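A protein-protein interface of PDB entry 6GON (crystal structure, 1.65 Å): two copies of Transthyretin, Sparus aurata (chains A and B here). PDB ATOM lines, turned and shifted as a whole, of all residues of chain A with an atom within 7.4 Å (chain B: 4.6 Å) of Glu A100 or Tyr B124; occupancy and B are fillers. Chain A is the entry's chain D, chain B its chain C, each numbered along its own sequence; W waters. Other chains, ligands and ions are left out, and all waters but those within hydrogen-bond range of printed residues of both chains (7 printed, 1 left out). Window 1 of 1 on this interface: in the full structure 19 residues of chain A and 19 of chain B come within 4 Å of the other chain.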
ATOM      1  N   ARG A  78      21.720   7.006  -8.411  1.00  0.00           N
ATOM      2  CA  ARG A  78      21.351   6.928  -7.008  1.00  0.00           C
ATOM      3  C   ARG A  78      22.520   6.286  -6.281  1.00  0.00           C
ATOM      4  O   ARG A  78      23.012   5.234  -6.698  1.00  0.00           O
ATOM      5  CB  ARG A  78      20.059   6.120  -6.842  1.00  0.00           C
ATOM      6  CG  ARG A  78      19.641   5.776  -5.436  1.00  0.00           C
ATOM      7  CD  ARG A  78      18.299   5.014  -5.446  1.00  0.00           C
ATOM      8  NE  ARG A  78      17.191   5.803  -6.008  1.00  0.00           N
ATOM      9  CZ  ARG A  78      16.386   6.590  -5.295  1.00  0.00           C
ATOM     10  NH1 ARG A  78      16.552   6.717  -3.996  1.00  0.00           N
ATOM     11  NH2 ARG A  78      15.414   7.266  -5.876  1.00  0.00           N
ATOM     12  N   VAL A  79      23.012   6.943  -5.236  1.00  0.00           N
ATOM     13  CA  VAL A  79      24.022   6.362  -4.370  1.00  0.00           C
ATOM     14  C   VAL A  79      23.373   6.174  -3.011  1.00  0.00           C
ATOM     15  O   VAL A  79      22.857   7.133  -2.418  1.00  0.00           O
ATOM     16  CB  VAL A  79      25.292   7.220  -4.283  1.00  0.00           C
ATOM     17  CG1 VAL A  79      26.287   6.514  -3.379  1.00  0.00           C
ATOM     18  CG2 VAL A  79      25.880   7.443  -5.668  1.00  0.00           C
ATOM     19  N   GLU A  80      23.353   4.917  -2.552  1.00  0.00           N
ATOM     20  CA  GLU A  80      22.686   4.505  -1.327  1.00  0.00           C
ATOM     21  C   GLU A  80      23.784   4.208  -0.323  1.00  0.00           C
ATOM     22  O   GLU A  80      24.617   3.320  -0.549  1.00  0.00           O
ATOM     23  CB  GLU A  80      21.812   3.272  -1.543  1.00  0.00           C
ATOM     24  CG  GLU A  80      21.073   2.886  -0.314  1.00  0.00           C
ATOM     25  CD  GLU A  80      20.362   1.538  -0.416  1.00  0.00           C
ATOM     26  OE1 GLU A  80      19.270   1.478  -1.022  1.00  0.00           O
ATOM     27  OE2 GLU A  80      20.904   0.543   0.106  1.00  0.00           O
ATOM     28  N   PHE A  81      23.814   4.980   0.765  1.00  0.00           N
ATOM     29  CA  PHE A  81      24.804   4.818   1.818  1.00  0.00           C
ATOM     30  C   PHE A  81      24.165   4.128   3.008  1.00  0.00           C
ATOM     31  O   PHE A  81      23.132   4.597   3.502  1.00  0.00           O
ATOM     32  CB  PHE A  81      25.330   6.179   2.275  1.00  0.00           C
ATOM     33  CG  PHE A  81      26.029   6.979   1.213  1.00  0.00           C
ATOM     34  CD1 PHE A  81      25.318   7.854   0.391  1.00  0.00           C
ATOM     35  CD2 PHE A  81      27.409   6.947   1.091  1.00  0.00           C
ATOM     36  CE1 PHE A  81      25.975   8.647  -0.542  1.00  0.00           C
ATOM     37  CE2 PHE A  81      28.060   7.745   0.158  1.00  0.00           C
ATOM     38  CZ  PHE A  81      27.337   8.584  -0.673  1.00  0.00           C
ATOM     39  N   THR A  83      24.092   4.068   6.232  1.00  0.00           N
ATOM     40  CA  THR A  83      24.446   4.809   7.434  1.00  0.00           C
ATOM     41  C   THR A  83      23.951   4.107   8.698  1.00  0.00           C
ATOM     42  O   THR A  83      24.550   4.258   9.768  1.00  0.00           O
ATOM     43  CB  THR A  83      23.873   6.218   7.354  1.00  0.00           C
ATOM     44  OG1 THR A  83      22.457   6.180   7.206  1.00  0.00           O
ATOM     45  CG2 THR A  83      24.425   6.984   6.183  1.00  0.00           C
ATOM     46  N   VAL A  98      18.703   4.710   5.864  1.00  0.00           N
ATOM     47  CA  VAL A  98      19.695   4.786   4.809  1.00  0.00           C
ATOM     48  C   VAL A  98      19.824   6.263   4.462  1.00  0.00           C
ATOM     49  O   VAL A  98      18.983   7.069   4.862  1.00  0.00           O
ATOM     50  CB  VAL A  98      19.224   3.944   3.592  1.00  0.00           C
ATOM     51  CG1 VAL A  98      17.981   4.592   2.952  1.00  0.00           C
ATOM     52  CG2 VAL A  98      20.301   3.764   2.608  1.00  0.00           C
ATOM     53  N   ALA A  99      20.888   6.635   3.746  1.00  0.00           N
ATOM     54  CA  ALA A  99      21.018   7.977   3.181  1.00  0.00           C
ATOM     55  C   ALA A  99      21.207   7.825   1.685  1.00  0.00           C
ATOM     56  O   ALA A  99      22.169   7.192   1.247  1.00  0.00           O
ATOM     57  CB  ALA A  99      22.198   8.746   3.772  1.00  0.00           C
ATOM     58  N   GLU A 100      20.298   8.398   0.901  1.00  0.00           N
ATOM     59  CA  GLU A 100      20.359   8.273  -0.545  1.00  0.00           C
ATOM     60  C   GLU A 100      20.627   9.620  -1.190  1.00  0.00           C
ATOM     61  O   GLU A 100      20.052  10.638  -0.790  1.00  0.00           O
ATOM     62  CB  GLU A 100      19.045   7.731  -1.109  1.00  0.00           C
ATOM     63  CG  GLU A 100      18.699   6.348  -0.636  1.00  0.00           C
ATOM     64  CD  GLU A 100      17.206   6.063  -0.753  1.00  0.00           C
ATOM     65  OE1 GLU A 100      16.382   6.812  -0.158  1.00  0.00           O
ATOM     66  OE2 GLU A 100      16.862   5.089  -1.445  1.00  0.00           O
ATOM     67  N   VAL A 101      21.484   9.612  -2.199  1.00  0.00           N
ATOM     68  CA  VAL A 101      21.828  10.813  -2.945  1.00  0.00           C
ATOM     69  C   VAL A 101      21.481  10.548  -4.408  1.00  0.00           C
ATOM     70  O   VAL A 101      22.007   9.606  -5.001  1.00  0.00           O
ATOM     71  CB  VAL A 101      23.308  11.177  -2.777  1.00  0.00           C
ATOM     72  CG1 VAL A 101      23.682  12.333  -3.682  1.00  0.00           C
ATOM     73  CG2 VAL A 101      23.603  11.552  -1.303  1.00  0.00           C
ATOM     74  N   VAL A 102      20.591  11.354  -4.980  1.00  0.00           N
ATOM     75  CA  VAL A 102      20.059  11.099  -6.330  1.00  0.00           C
ATOM     76  C   VAL A 102      20.317  12.338  -7.169  1.00  0.00           C
ATOM     77  O   VAL A 102      19.942  13.452  -6.771  1.00  0.00           O
ATOM     78  CB  VAL A 102      18.556  10.787  -6.305  1.00  0.00           C
ATOM     79  CG1 VAL A 102      18.099  10.312  -7.702  1.00  0.00           C
ATOM     80  CG2 VAL A 102      18.250   9.717  -5.299  1.00  0.00           C
ATOM     81  N   ALA A 116      29.875  14.403  -0.879  1.00  0.00           N
ATOM     82  CA  ALA A 116      30.353  14.504   0.487  1.00  0.00           C
ATOM     83  C   ALA A 116      29.180  14.307   1.419  1.00  0.00           C
ATOM     84  O   ALA A 116      28.053  14.738   1.129  1.00  0.00           O
ATOM     85  CB  ALA A 116      31.009  15.852   0.755  1.00  0.00           C
ATOM     86  N   LEU A 117      29.438  13.609   2.519  1.00  0.00           N
ATOM     87  CA  LEU A 117      28.386  13.242   3.450  1.00  0.00           C
ATOM     88  C   LEU A 117      28.936  13.366   4.860  1.00  0.00           C
ATOM     89  O   LEU A 117      29.941  12.727   5.188  1.00  0.00           O
ATOM     90  CB  LEU A 117      27.929  11.811   3.163  1.00  0.00           C
ATOM     91  CG  LEU A 117      26.778  11.243   3.928  1.00  0.00           C
ATOM     92  CD1 LEU A 117      25.509  12.026   3.616  1.00  0.00           C
ATOM     93  CD2 LEU A 117      26.605   9.776   3.506  1.00  0.00           C
ATOM     94  N   TYR A 124      22.171  14.168   8.773  1.00  0.00           N
ATOM     95  CA  TYR A 124      23.302  14.197   7.863  1.00  0.00           C
ATOM     96  C   TYR A 124      23.202  15.418   6.974  1.00  0.00           C
ATOM     97  O   TYR A 124      22.122  15.950   6.709  1.00  0.00           O
ATOM     98  CB  TYR A 124      23.462  12.918   7.030  1.00  0.00           C
ATOM     99  CG  TYR A 124      22.282  12.492   6.168  1.00  0.00           C
ATOM    100  CD1 TYR A 124      22.129  12.935   4.884  1.00  0.00           C
ATOM    101  CD2 TYR A 124      21.380  11.602   6.664  1.00  0.00           C
ATOM    102  CE1 TYR A 124      21.043  12.520   4.104  1.00  0.00           C
ATOM    103  CE2 TYR A 124      20.284  11.159   5.899  1.00  0.00           C
ATOM    104  CZ  TYR A 124      20.142  11.615   4.632  1.00  0.00           C
ATOM    105  OH  TYR A 124      19.058  11.193   3.881  1.00  0.00           O
ATOM    106  N   THR A 125      24.366  15.875   6.552  1.00  0.00           N
ATOM    107  CA  THR A 125      24.501  16.919   5.545  1.00  0.00           C
ATOM    108  C   THR A 125      25.140  16.300   4.325  1.00  0.00           C
ATOM    109  O   THR A 125      26.147  15.602   4.437  1.00  0.00           O
ATOM    110  CB  THR A 125      25.390  18.044   6.056  1.00  0.00           C
ATOM    111  OG1 THR A 125      24.758  18.683   7.164  1.00  0.00           O
ATOM    112  CG2 THR A 125      25.667  19.073   4.958  1.00  0.00           C
ATOM    113  N   THR A 126      24.589  16.568   3.149  1.00  0.00           N
ATOM    114  CA  THR A 126      25.241  16.082   1.945  1.00  0.00           C
ATOM    115  C   THR A 126      25.338  17.179   0.906  1.00  0.00           C
ATOM    116  O   THR A 126      24.356  17.880   0.632  1.00  0.00           O
ATOM    117  CB  THR A 126      24.551  14.855   1.363  1.00  0.00           C
ATOM    118  OG1 THR A 126      25.437  14.274   0.414  1.00  0.00           O
ATOM    119  CG2 THR A 126      23.208  15.171   0.687  1.00  0.00           C
ATOM    120  N   THR A 127      26.525  17.292   0.314  1.00  0.00           N
ATOM    121  CA  THR A 127      26.821  18.292  -0.705  1.00  0.00           C
ATOM    122  C   THR A 127      27.542  17.611  -1.855  1.00  0.00           C
ATOM    123  O   THR A 127      27.920  16.437  -1.793  1.00  0.00           O
ATOM    124  CB  THR A 127      27.621  19.485  -0.162  1.00  0.00           C
ATOM    125  OG1 THR A 127      27.535  20.575  -1.098  1.00  0.00           O
ATOM    126  CG2 THR A 127      29.054  19.134   0.052  1.00  0.00           C
ATOM    127  N   ALA A 128      27.659  18.340  -2.950  1.00  0.00           N
ATOM    128  CA  ALA A 128      28.378  17.832  -4.102  1.00  0.00           C
ATOM    129  C   ALA A 128      29.369  18.873  -4.577  1.00  0.00           C
ATOM    130  O   ALA A 128      29.112  20.073  -4.487  1.00  0.00           O
ATOM    131  CB  ALA A 128      27.407  17.495  -5.211  1.00  0.00           C
ATOM    132  N   ARG B  78       9.177   6.594   3.929  1.00  0.00           N
ATOM    133  CA  ARG B  78      10.008   7.408   3.049  1.00  0.00           C
ATOM    134  C   ARG B  78       9.271   8.701   2.779  1.00  0.00           C
ATOM    135  O   ARG B  78       8.123   8.674   2.323  1.00  0.00           O
ATOM    136  CB  ARG B  78      10.289   6.665   1.730  1.00  0.00           C
ATOM    137  CG  ARG B  78      10.977   7.475   0.627  1.00  0.00           C
ATOM    138  CD  ARG B  78      11.121   6.610  -0.639  1.00  0.00           C
ATOM    139  NE  ARG B  78      11.920   5.410  -0.353  1.00  0.00           N
ATOM    140  CZ  ARG B  78      13.221   5.269  -0.622  1.00  0.00           C
ATOM    141  NH1 ARG B  78      13.893   6.223  -1.216  1.00  0.00           N
ATOM    142  NH2 ARG B  78      13.847   4.149  -0.295  1.00  0.00           N
ATOM    143  N   HIS B  96      20.552  18.010  -6.820  1.00  0.00           N
ATOM    144  CA  HIS B  96      19.847  16.769  -6.525  1.00  0.00           C
ATOM    145  C   HIS B  96      18.544  16.671  -7.292  1.00  0.00           C
ATOM    146  O   HIS B  96      17.846  17.667  -7.473  1.00  0.00           O
ATOM    147  CB  HIS B  96      19.540  16.678  -5.044  1.00  0.00           C
ATOM    148  CG  HIS B  96      20.754  16.726  -4.184  1.00  0.00           C
ATOM    149  ND1 HIS B  96      21.286  17.911  -3.708  1.00  0.00           N
ATOM    150  CD2 HIS B  96      21.549  15.737  -3.719  1.00  0.00           C
ATOM    151  CE1 HIS B  96      22.364  17.643  -2.996  1.00  0.00           C
ATOM    152  NE2 HIS B  96      22.529  16.331  -2.959  1.00  0.00           N
ATOM    153  N   VAL B  98      16.042  14.884  -6.135  1.00  0.00           N
ATOM    154  CA  VAL B  98      15.046  14.780  -5.093  1.00  0.00           C
ATOM    155  C   VAL B  98      15.827  14.686  -3.785  1.00  0.00           C
ATOM    156  O   VAL B  98      17.048  14.466  -3.788  1.00  0.00           O
ATOM    157  CB  VAL B  98      14.148  13.536  -5.349  1.00  0.00           C
ATOM    158  CG1 VAL B  98      14.926  12.265  -5.176  1.00  0.00           C
ATOM    159  CG2 VAL B  98      12.953  13.550  -4.495  1.00  0.00           C
ATOM    160  N   ALA B  99      15.144  14.897  -2.665  1.00  0.00           N
ATOM    161  CA  ALA B  99      15.714  14.624  -1.347  1.00  0.00           C
ATOM    162  C   ALA B  99      14.797  13.651  -0.631  1.00  0.00           C
ATOM    163  O   ALA B  99      13.615  13.939  -0.446  1.00  0.00           O
ATOM    164  CB  ALA B  99      15.874  15.884  -0.504  1.00  0.00           C
ATOM    165  N   GLU B 100      15.331  12.502  -0.234  1.00  0.00           N
ATOM    166  CA  GLU B 100      14.544  11.470   0.421  1.00  0.00           C
ATOM    167  C   GLU B 100      15.017  11.262   1.847  1.00  0.00           C
ATOM    168  O   GLU B 100      16.223  11.212   2.107  1.00  0.00           O
ATOM    169  CB  GLU B 100      14.650  10.144  -0.320  1.00  0.00           C
ATOM    170  CG  GLU B 100      14.146  10.196  -1.736  1.00  0.00           C
ATOM    171  CD  GLU B 100      14.684   9.090  -2.617  1.00  0.00           C
ATOM    172  OE1 GLU B 100      13.840   8.345  -3.150  1.00  0.00           O
ATOM    173  OE2 GLU B 100      15.931   8.969  -2.793  1.00  0.00           O
ATOM    174  N   VAL B 102      14.400   8.544   4.868  1.00  0.00           N
ATOM    175  CA  VAL B 102      13.863   7.203   5.102  1.00  0.00           C
ATOM    176  C   VAL B 102      14.173   6.809   6.536  1.00  0.00           C
ATOM    177  O   VAL B 102      15.332   6.874   6.943  1.00  0.00           O
ATOM    178  CB  VAL B 102      14.484   6.192   4.120  1.00  0.00           C
ATOM    179  CG1 VAL B 102      13.837   4.820   4.278  1.00  0.00           C
ATOM    180  CG2 VAL B 102      14.379   6.665   2.703  1.00  0.00           C
ATOM    181  N   LEU B 117      14.582  20.053   7.245  1.00  0.00           N
ATOM    182  CA  LEU B 117      15.343  19.981   6.017  1.00  0.00           C
ATOM    183  C   LEU B 117      15.787  21.390   5.675  1.00  0.00           C
ATOM    184  O   LEU B 117      14.951  22.290   5.533  1.00  0.00           O
ATOM    185  CB  LEU B 117      14.487  19.388   4.901  1.00  0.00           C
ATOM    186  CG  LEU B 117      15.075  19.144   3.533  1.00  0.00           C
ATOM    187  CD1 LEU B 117      16.126  18.075   3.582  1.00  0.00           C
ATOM    188  CD2 LEU B 117      13.934  18.746   2.608  1.00  0.00           C
ATOM    189  N   LEU B 118      17.088  21.564   5.498  1.00  0.00           N
ATOM    190  CA  LEU B 118      17.695  22.846   5.174  1.00  0.00           C
ATOM    191  C   LEU B 118      18.280  22.756   3.775  1.00  0.00           C
ATOM    192  O   LEU B 118      19.198  21.960   3.527  1.00  0.00           O
ATOM    193  CB  LEU B 118      18.786  23.210   6.172  1.00  0.00           C
ATOM    194  CG  LEU B 118      19.488  24.523   5.874  1.00  0.00           C
ATOM    195  CD1 LEU B 118      18.608  25.736   6.077  1.00  0.00           C
ATOM    196  CD2 LEU B 118      20.699  24.583   6.766  1.00  0.00           C
ATOM    197  N   LEU B 119      17.739  23.552   2.853  1.00  0.00           N
ATOM    198  CA  LEU B 119      18.032  23.435   1.436  1.00  0.00           C
ATOM    199  C   LEU B 119      18.976  24.512   0.922  1.00  0.00           C
ATOM    200  O   LEU B 119      18.729  25.705   1.126  1.00  0.00           O
ATOM    201  CB  LEU B 119      16.737  23.529   0.642  1.00  0.00           C
ATOM    202  CG  LEU B 119      15.701  22.457   0.929  1.00  0.00           C
ATOM    203  CD1 LEU B 119      14.509  22.679  -0.007  1.00  0.00           C
ATOM    204  CD2 LEU B 119      16.287  21.052   0.774  1.00  0.00           C
ATOM    205  N   SER B 123      23.250  21.331  -1.820  1.00  0.00           N
ATOM    206  CA  SER B 123      23.432  20.694  -0.520  1.00  0.00           C
ATOM    207  C   SER B 123      22.115  20.676   0.235  1.00  0.00           C
ATOM    208  O   SER B 123      21.282  21.565   0.071  1.00  0.00           O
ATOM    209  CB  SER B 123      24.484  21.444   0.304  1.00  0.00           C
ATOM    210  OG  SER B 123      24.727  20.801   1.537  1.00  0.00           O
ATOM    211  N   TYR B 124      21.939  19.664   1.084  1.00  0.00           N
ATOM    212  CA  TYR B 124      20.893  19.762   2.084  1.00  0.00           C
ATOM    213  C   TYR B 124      21.339  19.084   3.372  1.00  0.00           C
ATOM    214  O   TYR B 124      22.192  18.193   3.377  1.00  0.00           O
ATOM    215  CB  TYR B 124      19.541  19.196   1.633  1.00  0.00           C
ATOM    216  CG  TYR B 124      19.516  17.754   1.156  1.00  0.00           C
ATOM    217  CD1 TYR B 124      19.290  16.711   2.025  1.00  0.00           C
ATOM    218  CD2 TYR B 124      19.696  17.473  -0.178  1.00  0.00           C
ATOM    219  CE1 TYR B 124      19.253  15.400   1.558  1.00  0.00           C
ATOM    220  CE2 TYR B 124      19.675  16.190  -0.654  1.00  0.00           C
ATOM    221  CZ  TYR B 124      19.445  15.165   0.206  1.00  0.00           C
ATOM    222  OH  TYR B 124      19.400  13.896  -0.320  1.00  0.00           O
ATOM    223  N   THR B 125      20.755  19.551   4.454  1.00  0.00           N
ATOM    224  CA  THR B 125      20.933  18.967   5.776  1.00  0.00           C
ATOM    225  C   THR B 125      19.575  18.484   6.235  1.00  0.00           C
ATOM    226  O   THR B 125      18.599  19.236   6.170  1.00  0.00           O
ATOM    227  CB  THR B 125      21.478  19.994   6.749  1.00  0.00           C
ATOM    228  OG1 THR B 125      22.803  20.378   6.362  1.00  0.00           O
ATOM    229  CG2 THR B 125      21.526  19.424   8.165  1.00  0.00           C
ATOM    230  N   THR B 126      19.542  17.317   6.800  1.00  0.00           N
ATOM    231  CA  THR B 126      18.298  16.901   7.386  1.00  0.00           C
ATOM    232  C   THR B 126      18.600  16.378   8.768  1.00  0.00           C
ATOM    233  O   THR B 126      19.688  15.862   9.029  1.00  0.00           O
ATOM    234  CB  THR B 126      17.591  15.894   6.501  1.00  0.00           C
ATOM    235  OG1 THR B 126      16.244  15.762   6.956  1.00  0.00           O
ATOM    236  CG2 THR B 126      18.323  14.539   6.453  1.00  0.00           C
HETATM  237  O   HOH W   1      17.240   9.061   4.687  1.00  0.00           O
HETATM  238  O   HOH W   2      14.418   5.397  -3.415  1.00  0.00           O
HETATM  239  O   HOH W   3      25.179  15.359  -2.307  1.00  0.00           O
HETATM  240  O   HOH W   4      17.556   8.526   1.740  1.00  0.00           O
HETATM  241  O   HOH W   5      17.302  11.256  -1.873  1.00  0.00           O
HETATM  242  O   HOH W   6      19.295  13.186  -2.999  1.00  0.00           O
HETATM  243  O   HOH W   7      18.703  11.729   1.299  1.00  0.00           O
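The guanidinium group (NH1) of Arg B78 is in salt-bridge range of the side-chain carboxylate (OE1) of Glu A100 (2.8 Å).
OG1 of Thr B125 is in hydrogen-bond range of OG1 of Thr A125 (2.7 Å).
N of Thr B126 sits at hydrogen-bond distance from O of Tyr A124 (2.9 Å).
OH of Tyr B124 lies within hydrogen-bond range of O of Glu A100.
The side-chain carboxylate (OE2) of Glu B100 lies close to the side-chain carboxylate (OE1) of Glu A100 (3.4 Å).
The guanidinium group of Arg A78 lies within salt-bridge range of the side-chain carboxylate of Glu B100 (2.6 Å).
The backbone carbonyl oxygen (O) of Tyr B124 sits at hydrogen-bond distance from the backbone NH (N) of Thr A126.
OG of Ser B123 lies within hydrogen-bond range of O of Thr A126 (3.1 Å).
The backbone carbonyl oxygen (O) of Glu B100 sits at hydrogen-bond distance from the side-chain hydroxyl (OH) of Tyr A124.
Of the 13 printed residues of chain B, 8 touch a printed residue of chain A.
Printed residues of chain B that touch a printed residue of chain A: Arg B78, His B96, Glu B100, Val B102, Ser B123, Tyr B124, Thr B125 and Thr B126.
Hydrophobic or aromatic side chains of chain B within 4 Å of the printed part of chain A: His B96, Val B102 and Tyr B124.
Along chain B the printed residues that touch a printed residue of chain A span positions 78 to 126.
Printed residues of chain A that touch a printed residue of chain B: Arg A78, Glu A100, Val A102, Tyr A124, Thr A125, Thr A126 and Thr A127.
Hydrophobic or aromatic side chains of chain A that line the printed part of chain B: Val A102 and Tyr A124.
Among the printed residues, 18 pairs touch across the chains.
Water W2 lies within hydrogen-bond range of the guanidinium group of Arg B78, the guanidinium group of Arg A78, the side-chain carboxylate of Glu B100 and the side-chain carboxylate of Glu A100.
Water W1 lies within hydrogen-bond range of O of Val A98 (2.7 Å), N of Val B102 (2.9 Å) and OH of Tyr A124 (2.9 Å).
Water W7 lies within hydrogen-bond range of the backbone carbonyl oxygen (O) of Glu B100 (2.7 Å), the side-chain hydroxyl (OH) of Tyr A124 (2.7 Å), the backbone carbonyl oxygen (O) of Glu A100 (2.7 Å) and the side-chain hydroxyl (OH) of Tyr B124 (2.8 Å).
Water W6 lies within hydrogen-bond range of O of Val B98 (2.7 Å), OH of Tyr B124 (2.8 Å), N of Val A102 (3.0 Å) and O of Glu A100 (3.5 Å).
Water W5 lies within hydrogen-bond range of OE2 of Glu B100 (2.8 Å) and O of Glu A100 (3.0 Å).
Water W3 lies within hydrogen-bond range of a ring nitrogen (NE2) of His B96, the side-chain hydroxyl of Thr A126 and the backbone carbonyl oxygen of Thr A127.
Printed residues of chain B within 4 Å of Glu A100: Arg B78, Glu B100, Val B102 and Tyr B124.
Of the printed residues of chain A, Tyr B124 touches Glu A100, Thr A125 and Thr A126.
Of the printed residues of chain B, Val A102 touches His B96 (3.3 Å) and Glu B100 (3.5 Å).
Printed residues of chain B within 4 Å of Thr A126: His B96 (3.9 Å), Ser B123 (3.1 Å) and Tyr B124 (2.9 Å).
Printed residues of chain A within 4 Å of Val B102: Glu A100 (3.5 Å).
The nearest printed residue of chain B that does not touch Glu A100 is Val B98 (5.7 Å).
The nearest printed residue of chain A that does not touch Tyr B124 is Tyr A124 (4.02 Å).
The nearest printed residue of chain B that does not touch Tyr A124 is Tyr B124 (4.02 Å).
Among the printed residues, merely in contact across the chains: Arg A78 with Arg B78 (3.9 Å), Glu A100 with Val B102 (3.5 Å), Val A102 with His B96 (3.3 Å), Val A102 with Glu B100 (3.5 Å), Tyr A124 with Thr B125 (3.4 Å), Thr A125 with Ser B123 (3.9 Å), Thr A125 with Tyr B124 (3.4 Å), Thr A126 with His B96 (3.9 Å) and Thr A127 with Ser B123 (3.5 Å).
Arg A78 touches its own counterpart, Arg B78.
Glu A100 touches Val B102, and with the chains exchanged Val A102 touches Glu B100.
Tyr A124 touches Thr B125, and with the chains exchanged Thr A125 touches Tyr B124.
Tyr A124 touches Thr B126, and with the chains exchanged Thr A126 touches Tyr B124.
Positions printed for both chains: 78, 98, 99, 100, 102, 117, 124, 125 and 126.
Of the 18 pairs that touch across the chains among the printed residues, 13 have their exchanged pair printed and touching as well.
NH1 of Arg B78 is in salt-bridge range of OE1 of Glu B100 (2.9 Å).
N of Ala A116 sits at hydrogen-bond distance from O of Thr A127 (3.0 Å).
NH1 of Arg A78 is in salt-bridge range of OE2 of Glu A100.
The backbone carbonyl oxygen (O) of Ala A116 lies within hydrogen-bond range of the side-chain hydroxyl (OG1) of Thr A126, 2.8 Å away.
N of Leu B118 is in hydrogen-bond range of O of Thr B125, at 2.9 Å.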
